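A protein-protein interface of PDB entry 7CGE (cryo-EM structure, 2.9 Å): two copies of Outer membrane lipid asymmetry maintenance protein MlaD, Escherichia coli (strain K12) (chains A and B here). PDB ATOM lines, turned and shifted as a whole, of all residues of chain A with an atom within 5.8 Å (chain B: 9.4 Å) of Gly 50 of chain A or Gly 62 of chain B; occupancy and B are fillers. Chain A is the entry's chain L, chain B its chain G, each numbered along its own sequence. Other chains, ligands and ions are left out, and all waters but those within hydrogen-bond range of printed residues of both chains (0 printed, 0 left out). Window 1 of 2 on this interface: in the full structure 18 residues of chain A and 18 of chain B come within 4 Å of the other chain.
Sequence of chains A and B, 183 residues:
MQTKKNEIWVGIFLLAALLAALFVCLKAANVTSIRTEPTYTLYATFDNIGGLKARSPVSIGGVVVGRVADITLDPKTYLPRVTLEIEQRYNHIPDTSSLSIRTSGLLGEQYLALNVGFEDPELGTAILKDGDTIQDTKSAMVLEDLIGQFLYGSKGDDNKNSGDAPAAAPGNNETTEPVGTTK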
ATOM      1  N   ASN A  48      20.958 -27.247  -3.684  1.00  0.00           N
ATOM      2  CA  ASN A  48      19.597 -27.276  -3.171  1.00  0.00           C
ATOM      3  C   ASN A  48      19.398 -28.582  -2.426  1.00  0.00           C
ATOM      4  O   ASN A  48      19.732 -29.649  -2.948  1.00  0.00           O
ATOM      5  CB  ASN A  48      18.579 -27.159  -4.302  1.00  0.00           C
ATOM      6  CG  ASN A  48      17.168 -27.063  -3.797  1.00  0.00           C
ATOM      7  OD1 ASN A  48      16.899 -26.411  -2.794  1.00  0.00           O
ATOM      8  ND2 ASN A  48      16.252 -27.715  -4.490  1.00  0.00           N
ATOM      9  N   ILE A  49      18.858 -28.504  -1.212  1.00  0.00           N
ATOM     10  CA  ILE A  49      18.632 -29.685  -0.393  1.00  0.00           C
ATOM     11  C   ILE A  49      17.167 -29.940  -0.124  1.00  0.00           C
ATOM     12  O   ILE A  49      16.849 -30.932   0.540  1.00  0.00           O
ATOM     13  CB  ILE A  49      19.370 -29.593   0.952  1.00  0.00           C
ATOM     14  CG1 ILE A  49      18.733 -28.499   1.789  1.00  0.00           C
ATOM     15  CG2 ILE A  49      20.829 -29.319   0.747  1.00  0.00           C
ATOM     16  CD1 ILE A  49      19.048 -28.610   3.205  1.00  0.00           C
ATOM     17  N   GLY A  50      16.270 -29.102  -0.643  1.00  0.00           N
ATOM     18  CA  GLY A  50      14.938 -28.838  -0.119  1.00  0.00           C
ATOM     19  C   GLY A  50      14.070 -29.972   0.375  1.00  0.00           C
ATOM     20  O   GLY A  50      13.726 -30.880  -0.381  1.00  0.00           O
ATOM     21  N   GLY A  51      13.723 -29.933   1.655  1.00  0.00           N
ATOM     22  CA  GLY A  51      12.942 -30.968   2.287  1.00  0.00           C
ATOM     23  C   GLY A  51      13.720 -31.810   3.265  1.00  0.00           C
ATOM     24  O   GLY A  51      13.116 -32.450   4.130  1.00  0.00           O
ATOM     25  N   LEU A  52      15.042 -31.828   3.150  1.00  0.00           N
ATOM     26  CA  LEU A  52      15.878 -32.549   4.094  1.00  0.00           C
ATOM     27  C   LEU A  52      15.901 -31.818   5.426  1.00  0.00           C
ATOM     28  O   LEU A  52      16.079 -30.601   5.473  1.00  0.00           O
ATOM     29  CB  LEU A  52      17.286 -32.683   3.533  1.00  0.00           C
ATOM     30  CG  LEU A  52      18.224 -33.726   4.115  1.00  0.00           C
ATOM     31  CD1 LEU A  52      17.916 -35.065   3.540  1.00  0.00           C
ATOM     32  CD2 LEU A  52      19.640 -33.344   3.801  1.00  0.00           C
ATOM     33  N   PRO A  80      24.021 -24.446   1.207  1.00  0.00           N
ATOM     34  CA  PRO A  80      23.738 -25.247   2.397  1.00  0.00           C
ATOM     35  C   PRO A  80      24.849 -26.237   2.699  1.00  0.00           C
ATOM     36  O   PRO A  80      25.470 -26.816   1.808  1.00  0.00           O
ATOM     37  CB  PRO A  80      22.442 -25.979   2.024  1.00  0.00           C
ATOM     38  CG  PRO A  80      21.968 -25.346   0.769  1.00  0.00           C
ATOM     39  CD  PRO A  80      23.176 -24.862   0.081  1.00  0.00           C
ATOM     40  N   ILE A 101      20.213 -36.691  -3.174  1.00  0.00           N
ATOM     41  CA  ILE A 101      19.046 -36.493  -2.328  1.00  0.00           C
ATOM     42  C   ILE A 101      17.832 -37.061  -3.042  1.00  0.00           C
ATOM     43  O   ILE A 101      17.460 -36.587  -4.120  1.00  0.00           O
ATOM     44  CB  ILE A 101      18.861 -35.012  -1.986  1.00  0.00           C
ATOM     45  CG1 ILE A 101      20.160 -34.468  -1.406  1.00  0.00           C
ATOM     46  CG2 ILE A 101      17.743 -34.838  -1.013  1.00  0.00           C
ATOM     47  CD1 ILE A 101      20.063 -33.102  -0.825  1.00  0.00           C
ATOM     48  N   GLY A 108       6.750 -34.579   0.790  1.00  0.00           N
ATOM     49  CA  GLY A 108       7.851 -33.680   0.531  1.00  0.00           C
ATOM     50  C   GLY A 108       9.123 -33.927   1.308  1.00  0.00           C
ATOM     51  O   GLY A 108      10.047 -33.117   1.230  1.00  0.00           O
ATOM     52  N   GLN A 110      12.721 -35.929   2.403  1.00  0.00           N
ATOM     53  CA  GLN A 110      13.856 -36.415   1.635  1.00  0.00           C
ATOM     54  C   GLN A 110      14.704 -37.326   2.501  1.00  0.00           C
ATOM     55  O   GLN A 110      14.481 -37.462   3.703  1.00  0.00           O
ATOM     56  CB  GLN A 110      14.756 -35.291   1.109  1.00  0.00           C
ATOM     57  CG  GLN A 110      14.098 -34.061   0.530  1.00  0.00           C
ATOM     58  CD  GLN A 110      13.599 -34.256  -0.868  1.00  0.00           C
ATOM     59  OE1 GLN A 110      12.468 -33.917  -1.180  1.00  0.00           O
ATOM     60  NE2 GLN A 110      14.436 -34.802  -1.725  1.00  0.00           N
ATOM     61  N   ALA A 140      19.253 -31.953  -4.655  1.00  0.00           N
ATOM     62  CA  ALA A 140      17.850 -32.343  -4.635  1.00  0.00           C
ATOM     63  C   ALA A 140      17.142 -31.698  -5.812  1.00  0.00           C
ATOM     64  O   ALA A 140      17.231 -30.484  -6.002  1.00  0.00           O
ATOM     65  CB  ALA A 140      17.178 -31.920  -3.333  1.00  0.00           C
ATOM     66  N   PRO B  57       7.013 -20.318   4.931  1.00  0.00           N
ATOM     67  CA  PRO B  57       8.450 -20.039   4.955  1.00  0.00           C
ATOM     68  C   PRO B  57       9.006 -19.485   3.655  1.00  0.00           C
ATOM     69  O   PRO B  57       8.454 -19.675   2.571  1.00  0.00           O
ATOM     70  CB  PRO B  57       9.058 -21.413   5.249  1.00  0.00           C
ATOM     71  CG  PRO B  57       8.080 -22.357   4.714  1.00  0.00           C
ATOM     72  CD  PRO B  57       6.754 -21.764   5.028  1.00  0.00           C
ATOM     73  N   VAL B  58      10.126 -18.777   3.796  1.00  0.00           N
ATOM     74  CA  VAL B  58      11.004 -18.418   2.690  1.00  0.00           C
ATOM     75  C   VAL B  58      12.261 -19.256   2.844  1.00  0.00           C
ATOM     76  O   VAL B  58      12.712 -19.499   3.967  1.00  0.00           O
ATOM     77  CB  VAL B  58      11.347 -16.915   2.684  1.00  0.00           C
ATOM     78  CG1 VAL B  58      11.926 -16.498   1.345  1.00  0.00           C
ATOM     79  CG2 VAL B  58      10.138 -16.098   3.010  1.00  0.00           C
ATOM     80  N   SER B  59      12.820 -19.713   1.733  1.00  0.00           N
ATOM     81  CA  SER B  59      13.962 -20.602   1.816  1.00  0.00           C
ATOM     82  C   SER B  59      15.007 -20.233   0.782  1.00  0.00           C
ATOM     83  O   SER B  59      14.675 -19.922  -0.361  1.00  0.00           O
ATOM     84  CB  SER B  59      13.551 -22.059   1.613  1.00  0.00           C
ATOM     85  OG  SER B  59      13.202 -22.301   0.265  1.00  0.00           O
ATOM     86  N   ILE B  60      16.270 -20.288   1.185  1.00  0.00           N
ATOM     87  CA  ILE B  60      17.398 -20.198   0.267  1.00  0.00           C
ATOM     88  C   ILE B  60      18.049 -21.568   0.239  1.00  0.00           C
ATOM     89  O   ILE B  60      18.567 -22.035   1.259  1.00  0.00           O
ATOM     90  CB  ILE B  60      18.407 -19.124   0.683  1.00  0.00           C
ATOM     91  CG1 ILE B  60      17.696 -17.828   1.042  1.00  0.00           C
ATOM     92  CG2 ILE B  60      19.409 -18.895  -0.430  1.00  0.00           C
ATOM     93  CD1 ILE B  60      18.623 -16.772   1.550  1.00  0.00           C
ATOM     94  N   GLY B  61      17.992 -22.234  -0.909  1.00  0.00           N
ATOM     95  CA  GLY B  61      18.570 -23.552  -1.060  1.00  0.00           C
ATOM     96  C   GLY B  61      17.892 -24.663  -0.291  1.00  0.00           C
ATOM     97  O   GLY B  61      18.383 -25.795  -0.321  1.00  0.00           O
ATOM     98  N   GLY B  62      16.782 -24.392   0.387  1.00  0.00           N
ATOM     99  CA  GLY B  62      16.123 -25.349   1.248  1.00  0.00           C
ATOM    100  C   GLY B  62      16.066 -24.943   2.703  1.00  0.00           C
ATOM    101  O   GLY B  62      15.224 -25.465   3.443  1.00  0.00           O
ATOM    102  N   VAL B  63      16.918 -24.025   3.144  1.00  0.00           N
ATOM    103  CA  VAL B  63      17.007 -23.656   4.552  1.00  0.00           C
ATOM    104  C   VAL B  63      16.114 -22.449   4.797  1.00  0.00           C
ATOM    105  O   VAL B  63      16.157 -21.479   4.037  1.00  0.00           O
ATOM    106  CB  VAL B  63      18.460 -23.350   4.940  1.00  0.00           C
ATOM    107  CG1 VAL B  63      18.584 -23.132   6.432  1.00  0.00           C
ATOM    108  CG2 VAL B  63      19.378 -24.443   4.462  1.00  0.00           C
ATOM    109  N   VAL B  64      15.322 -22.495   5.866  1.00  0.00           N
ATOM    110  CA  VAL B  64      14.337 -21.452   6.137  1.00  0.00           C
ATOM    111  C   VAL B  64      15.041 -20.189   6.618  1.00  0.00           C
ATOM    112  O   VAL B  64      15.754 -20.203   7.627  1.00  0.00           O
ATOM    113  CB  VAL B  64      13.306 -21.932   7.164  1.00  0.00           C
ATOM    114  CG1 VAL B  64      12.439 -20.783   7.627  1.00  0.00           C
ATOM    115  CG2 VAL B  64      12.450 -23.022   6.572  1.00  0.00           C
ATOM    116  N   VAL B  65      14.836 -19.087   5.899  1.00  0.00           N
ATOM    117  CA  VAL B  65      15.421 -17.801   6.258  1.00  0.00           C
ATOM    118  C   VAL B  65      14.385 -16.755   6.626  1.00  0.00           C
ATOM    119  O   VAL B  65      14.768 -15.633   6.979  1.00  0.00           O
ATOM    120  CB  VAL B  65      16.327 -17.255   5.133  1.00  0.00           C
ATOM    121  CG1 VAL B  65      17.367 -18.269   4.756  1.00  0.00           C
ATOM    122  CG2 VAL B  65      15.505 -16.880   3.935  1.00  0.00           C
ATOM    123  N   GLY B  66      13.097 -17.060   6.554  1.00  0.00           N
ATOM    124  CA  GLY B  66      12.099 -16.062   6.888  1.00  0.00           C
ATOM    125  C   GLY B  66      10.708 -16.531   6.531  1.00  0.00           C
ATOM    126  O   GLY B  66      10.511 -17.613   5.971  1.00  0.00           O
ATOM    127  N   ARG B 102       6.902 -22.511  -4.939  1.00  0.00           N
ATOM    128  CA  ARG B 102       7.028 -23.936  -5.184  1.00  0.00           C
ATOM    129  C   ARG B 102       6.187 -24.709  -4.182  1.00  0.00           C
ATOM    130  O   ARG B 102       5.665 -24.151  -3.217  1.00  0.00           O
ATOM    131  CB  ARG B 102       8.490 -24.368  -5.113  1.00  0.00           C
ATOM    132  CG  ARG B 102       9.301 -23.873  -6.273  1.00  0.00           C
ATOM    133  CD  ARG B 102      10.746 -24.202  -6.083  1.00  0.00           C
ATOM    134  NE  ARG B 102      11.510 -24.015  -7.307  1.00  0.00           N
ATOM    135  CZ  ARG B 102      12.822 -23.821  -7.331  1.00  0.00           C
ATOM    136  NH1 ARG B 102      13.502 -23.784  -6.195  1.00  0.00           N
ATOM    137  NH2 ARG B 102      13.450 -23.661  -8.485  1.00  0.00           N
ATOM    138  N   THR B 103       6.071 -26.016  -4.405  1.00  0.00           N
ATOM    139  CA  THR B 103       5.002 -26.774  -3.780  1.00  0.00           C
ATOM    140  C   THR B 103       5.430 -27.837  -2.784  1.00  0.00           C
ATOM    141  O   THR B 103       4.547 -28.515  -2.249  1.00  0.00           O
ATOM    142  CB  THR B 103       4.135 -27.450  -4.841  1.00  0.00           C
ATOM    143  OG1 THR B 103       3.007 -28.050  -4.199  1.00  0.00           O
ATOM    144  CG2 THR B 103       4.923 -28.520  -5.558  1.00  0.00           C
ATOM    145  N   SER B 104       6.732 -28.022  -2.545  1.00  0.00           N
ATOM    146  CA  SER B 104       7.288 -28.883  -1.487  1.00  0.00           C
ATOM    147  C   SER B 104       6.820 -30.335  -1.618  1.00  0.00           C
ATOM    148  O   SER B 104       6.047 -30.853  -0.816  1.00  0.00           O
ATOM    149  CB  SER B 104       6.960 -28.342  -0.093  1.00  0.00           C
ATOM    150  OG  SER B 104       6.923 -29.390   0.853  1.00  0.00           O
ATOM    151  N   GLY B 105       7.298 -30.974  -2.671  1.00  0.00           N
ATOM    152  CA  GLY B 105       6.892 -32.334  -2.917  1.00  0.00           C
ATOM    153  C   GLY B 105       5.815 -32.383  -3.969  1.00  0.00           C
ATOM    154  O   GLY B 105       6.000 -31.885  -5.080  1.00  0.00           O
ATOM    155  N   GLU B 109       2.978 -28.391   1.594  1.00  0.00           N
ATOM    156  CA  GLU B 109       2.691 -26.977   1.753  1.00  0.00           C
ATOM    157  C   GLU B 109       3.395 -26.169   0.670  1.00  0.00           C
ATOM    158  O   GLU B 109       4.207 -26.680  -0.094  1.00  0.00           O
ATOM    159  CB  GLU B 109       3.105 -26.517   3.151  1.00  0.00           C
ATOM    160  CG  GLU B 109       4.563 -26.795   3.510  1.00  0.00           C
ATOM    161  CD  GLU B 109       5.481 -25.635   3.210  1.00  0.00           C
ATOM    162  OE1 GLU B 109       4.975 -24.501   3.103  1.00  0.00           O
ATOM    163  OE2 GLU B 109       6.705 -25.849   3.094  1.00  0.00           O
ATOM    164  N   TYR B 111       5.643 -22.743  -0.512  1.00  0.00           N
ATOM    165  CA  TYR B 111       6.706 -21.922   0.053  1.00  0.00           C
ATOM    166  C   TYR B 111       7.360 -21.086  -1.040  1.00  0.00           C
ATOM    167  O   TYR B 111       7.149 -21.308  -2.235  1.00  0.00           O
ATOM    168  CB  TYR B 111       7.754 -22.787   0.769  1.00  0.00           C
ATOM    169  CG  TYR B 111       8.653 -23.576  -0.159  1.00  0.00           C
ATOM    170  CD1 TYR B 111       8.207 -24.731  -0.778  1.00  0.00           C
ATOM    171  CD2 TYR B 111       9.950 -23.168  -0.408  1.00  0.00           C
ATOM    172  CE1 TYR B 111       9.022 -25.444  -1.625  1.00  0.00           C
ATOM    173  CE2 TYR B 111      10.767 -23.873  -1.254  1.00  0.00           C
ATOM    174  CZ  TYR B 111      10.298 -25.010  -1.858  1.00  0.00           C
ATOM    175  OH  TYR B 111      11.112 -25.726  -2.702  1.00  0.00           O
ATOM    176  N   LEU B 112       8.180 -20.126  -0.613  1.00  0.00           N
ATOM    177  CA  LEU B 112       8.864 -19.196  -1.505  1.00  0.00           C
ATOM    178  C   LEU B 112      10.334 -19.572  -1.633  1.00  0.00           C
ATOM    179  O   LEU B 112      11.051 -19.628  -0.632  1.00  0.00           O
ATOM    180  CB  LEU B 112       8.740 -17.767  -0.987  1.00  0.00           C
ATOM    181  CG  LEU B 112       7.548 -16.985  -1.513  1.00  0.00           C
ATOM    182  CD1 LEU B 112       7.293 -15.790  -0.646  1.00  0.00           C
ATOM    183  CD2 LEU B 112       7.817 -16.558  -2.935  1.00  0.00           C
ATOM    184  N   ALA B 113      10.787 -19.788  -2.861  1.00  0.00           N
ATOM    185  CA  ALA B 113      12.154 -20.228  -3.121  1.00  0.00           C
ATOM    186  C   ALA B 113      12.982 -19.021  -3.539  1.00  0.00           C
ATOM    187  O   ALA B 113      13.120 -18.716  -4.723  1.00  0.00           O
ATOM    188  CB  ALA B 113      12.182 -21.314  -4.184  1.00  0.00           C
ATOM    189  N   LEU B 114      13.560 -18.346  -2.550  1.00  0.00           N
ATOM    190  CA  LEU B 114      14.376 -17.161  -2.785  1.00  0.00           C
ATOM    191  C   LEU B 114      15.713 -17.572  -3.384  1.00  0.00           C
ATOM    192  O   LEU B 114      16.565 -18.138  -2.697  1.00  0.00           O
ATOM    193  CB  LEU B 114      14.556 -16.398  -1.477  1.00  0.00           C
ATOM    194  CG  LEU B 114      15.561 -15.254  -1.342  1.00  0.00           C
ATOM    195  CD1 LEU B 114      15.415 -14.225  -2.437  1.00  0.00           C
ATOM    196  CD2 LEU B 114      15.365 -14.606   0.008  1.00  0.00           C
ATOM    197  N   ASN B 115      15.892 -17.298  -4.666  1.00  0.00           N
ATOM    198  CA  ASN B 115      17.147 -17.570  -5.344  1.00  0.00           C
ATOM    199  C   ASN B 115      18.060 -16.368  -5.179  1.00  0.00           C
ATOM    200  O   ASN B 115      17.622 -15.226  -5.323  1.00  0.00           O
ATOM    201  CB  ASN B 115      16.907 -17.860  -6.822  1.00  0.00           C
ATOM    202  CG  ASN B 115      18.110 -18.469  -7.499  1.00  0.00           C
ATOM    203  OD1 ASN B 115      19.138 -18.713  -6.870  1.00  0.00           O
ATOM    204  ND2 ASN B 115      17.989 -18.724  -8.791  1.00  0.00           N
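The backbone carbonyl oxygen (O) of Gly 61 of chain B sits close to the side-chain amide oxygen (OD1) of Asn 48 of chain A.
O of Gly 61 of chain B is in hydrogen-bond range of N of Ile 49 of chain A (2.9 Å).
The side-chain amide oxygen (OE1) of Gln 110 of chain A sits close to the backbone carbonyl oxygen (O) of Gly 50 of chain A (3.4 Å).
O of Asn 48 of chain A sits at hydrogen-bond distance from N of Ala 140 of chain A (2.9 Å).
Of chain A, only Asn 48 and Gly 50 come within 4 Å of Gly 62 of chain B.
Of the printed residues of chain B, Gly 108 of chain A touches Ser 104 (3.6 Å) and Gly 105 (3.8 Å).
Of the printed residues of chain A, Gly 105 of chain B touches Gly 108 (3.8 Å).
Of the printed residues of chain A, Gly 61 of chain B touches Asn 48 (2.9 Å), Ile 49 (2.9 Å), Gly 50 (3.9 Å) and Pro 80 (3.8 Å).
Of the printed residues of chain B, Asn 48 of chain A touches Gly 61 and Gly 62.
Printed residues of chain A within 4 Å of Ser 104 of chain B: Gly 108 (3.6 Å).
Val 58 of chain B touches none of the printed residues of chain A.
No position is printed for both chains.
Of the 8 pairs that touch across the chains among the printed residues, none has its exchanged pair printed and touching as well.
Gly 62 of chain B touches Asn 48 of chain A (N to OD1, 3.8 Å).
Gly 61 of chain B touches Gly 50 of chain A.
Gly 50 of chain A touches Gly 62 of chain B.
Gly 61 of chain B touches Pro 80 of chain A (O to CG, 3.8 Å).
Gly 108 of chain A touches Ser 104 of chain B.
Gly 108 of chain A touches Gly 105 of chain B.
Printed residues of chain B that touch a printed residue of chain A: Gly 61, Gly 62, Ser 104 and Gly 105.
Among the printed residues, no Asp or Glu carboxylate lies within 4 Å of a Lys or Arg side-chain nitrogen of the other chain.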
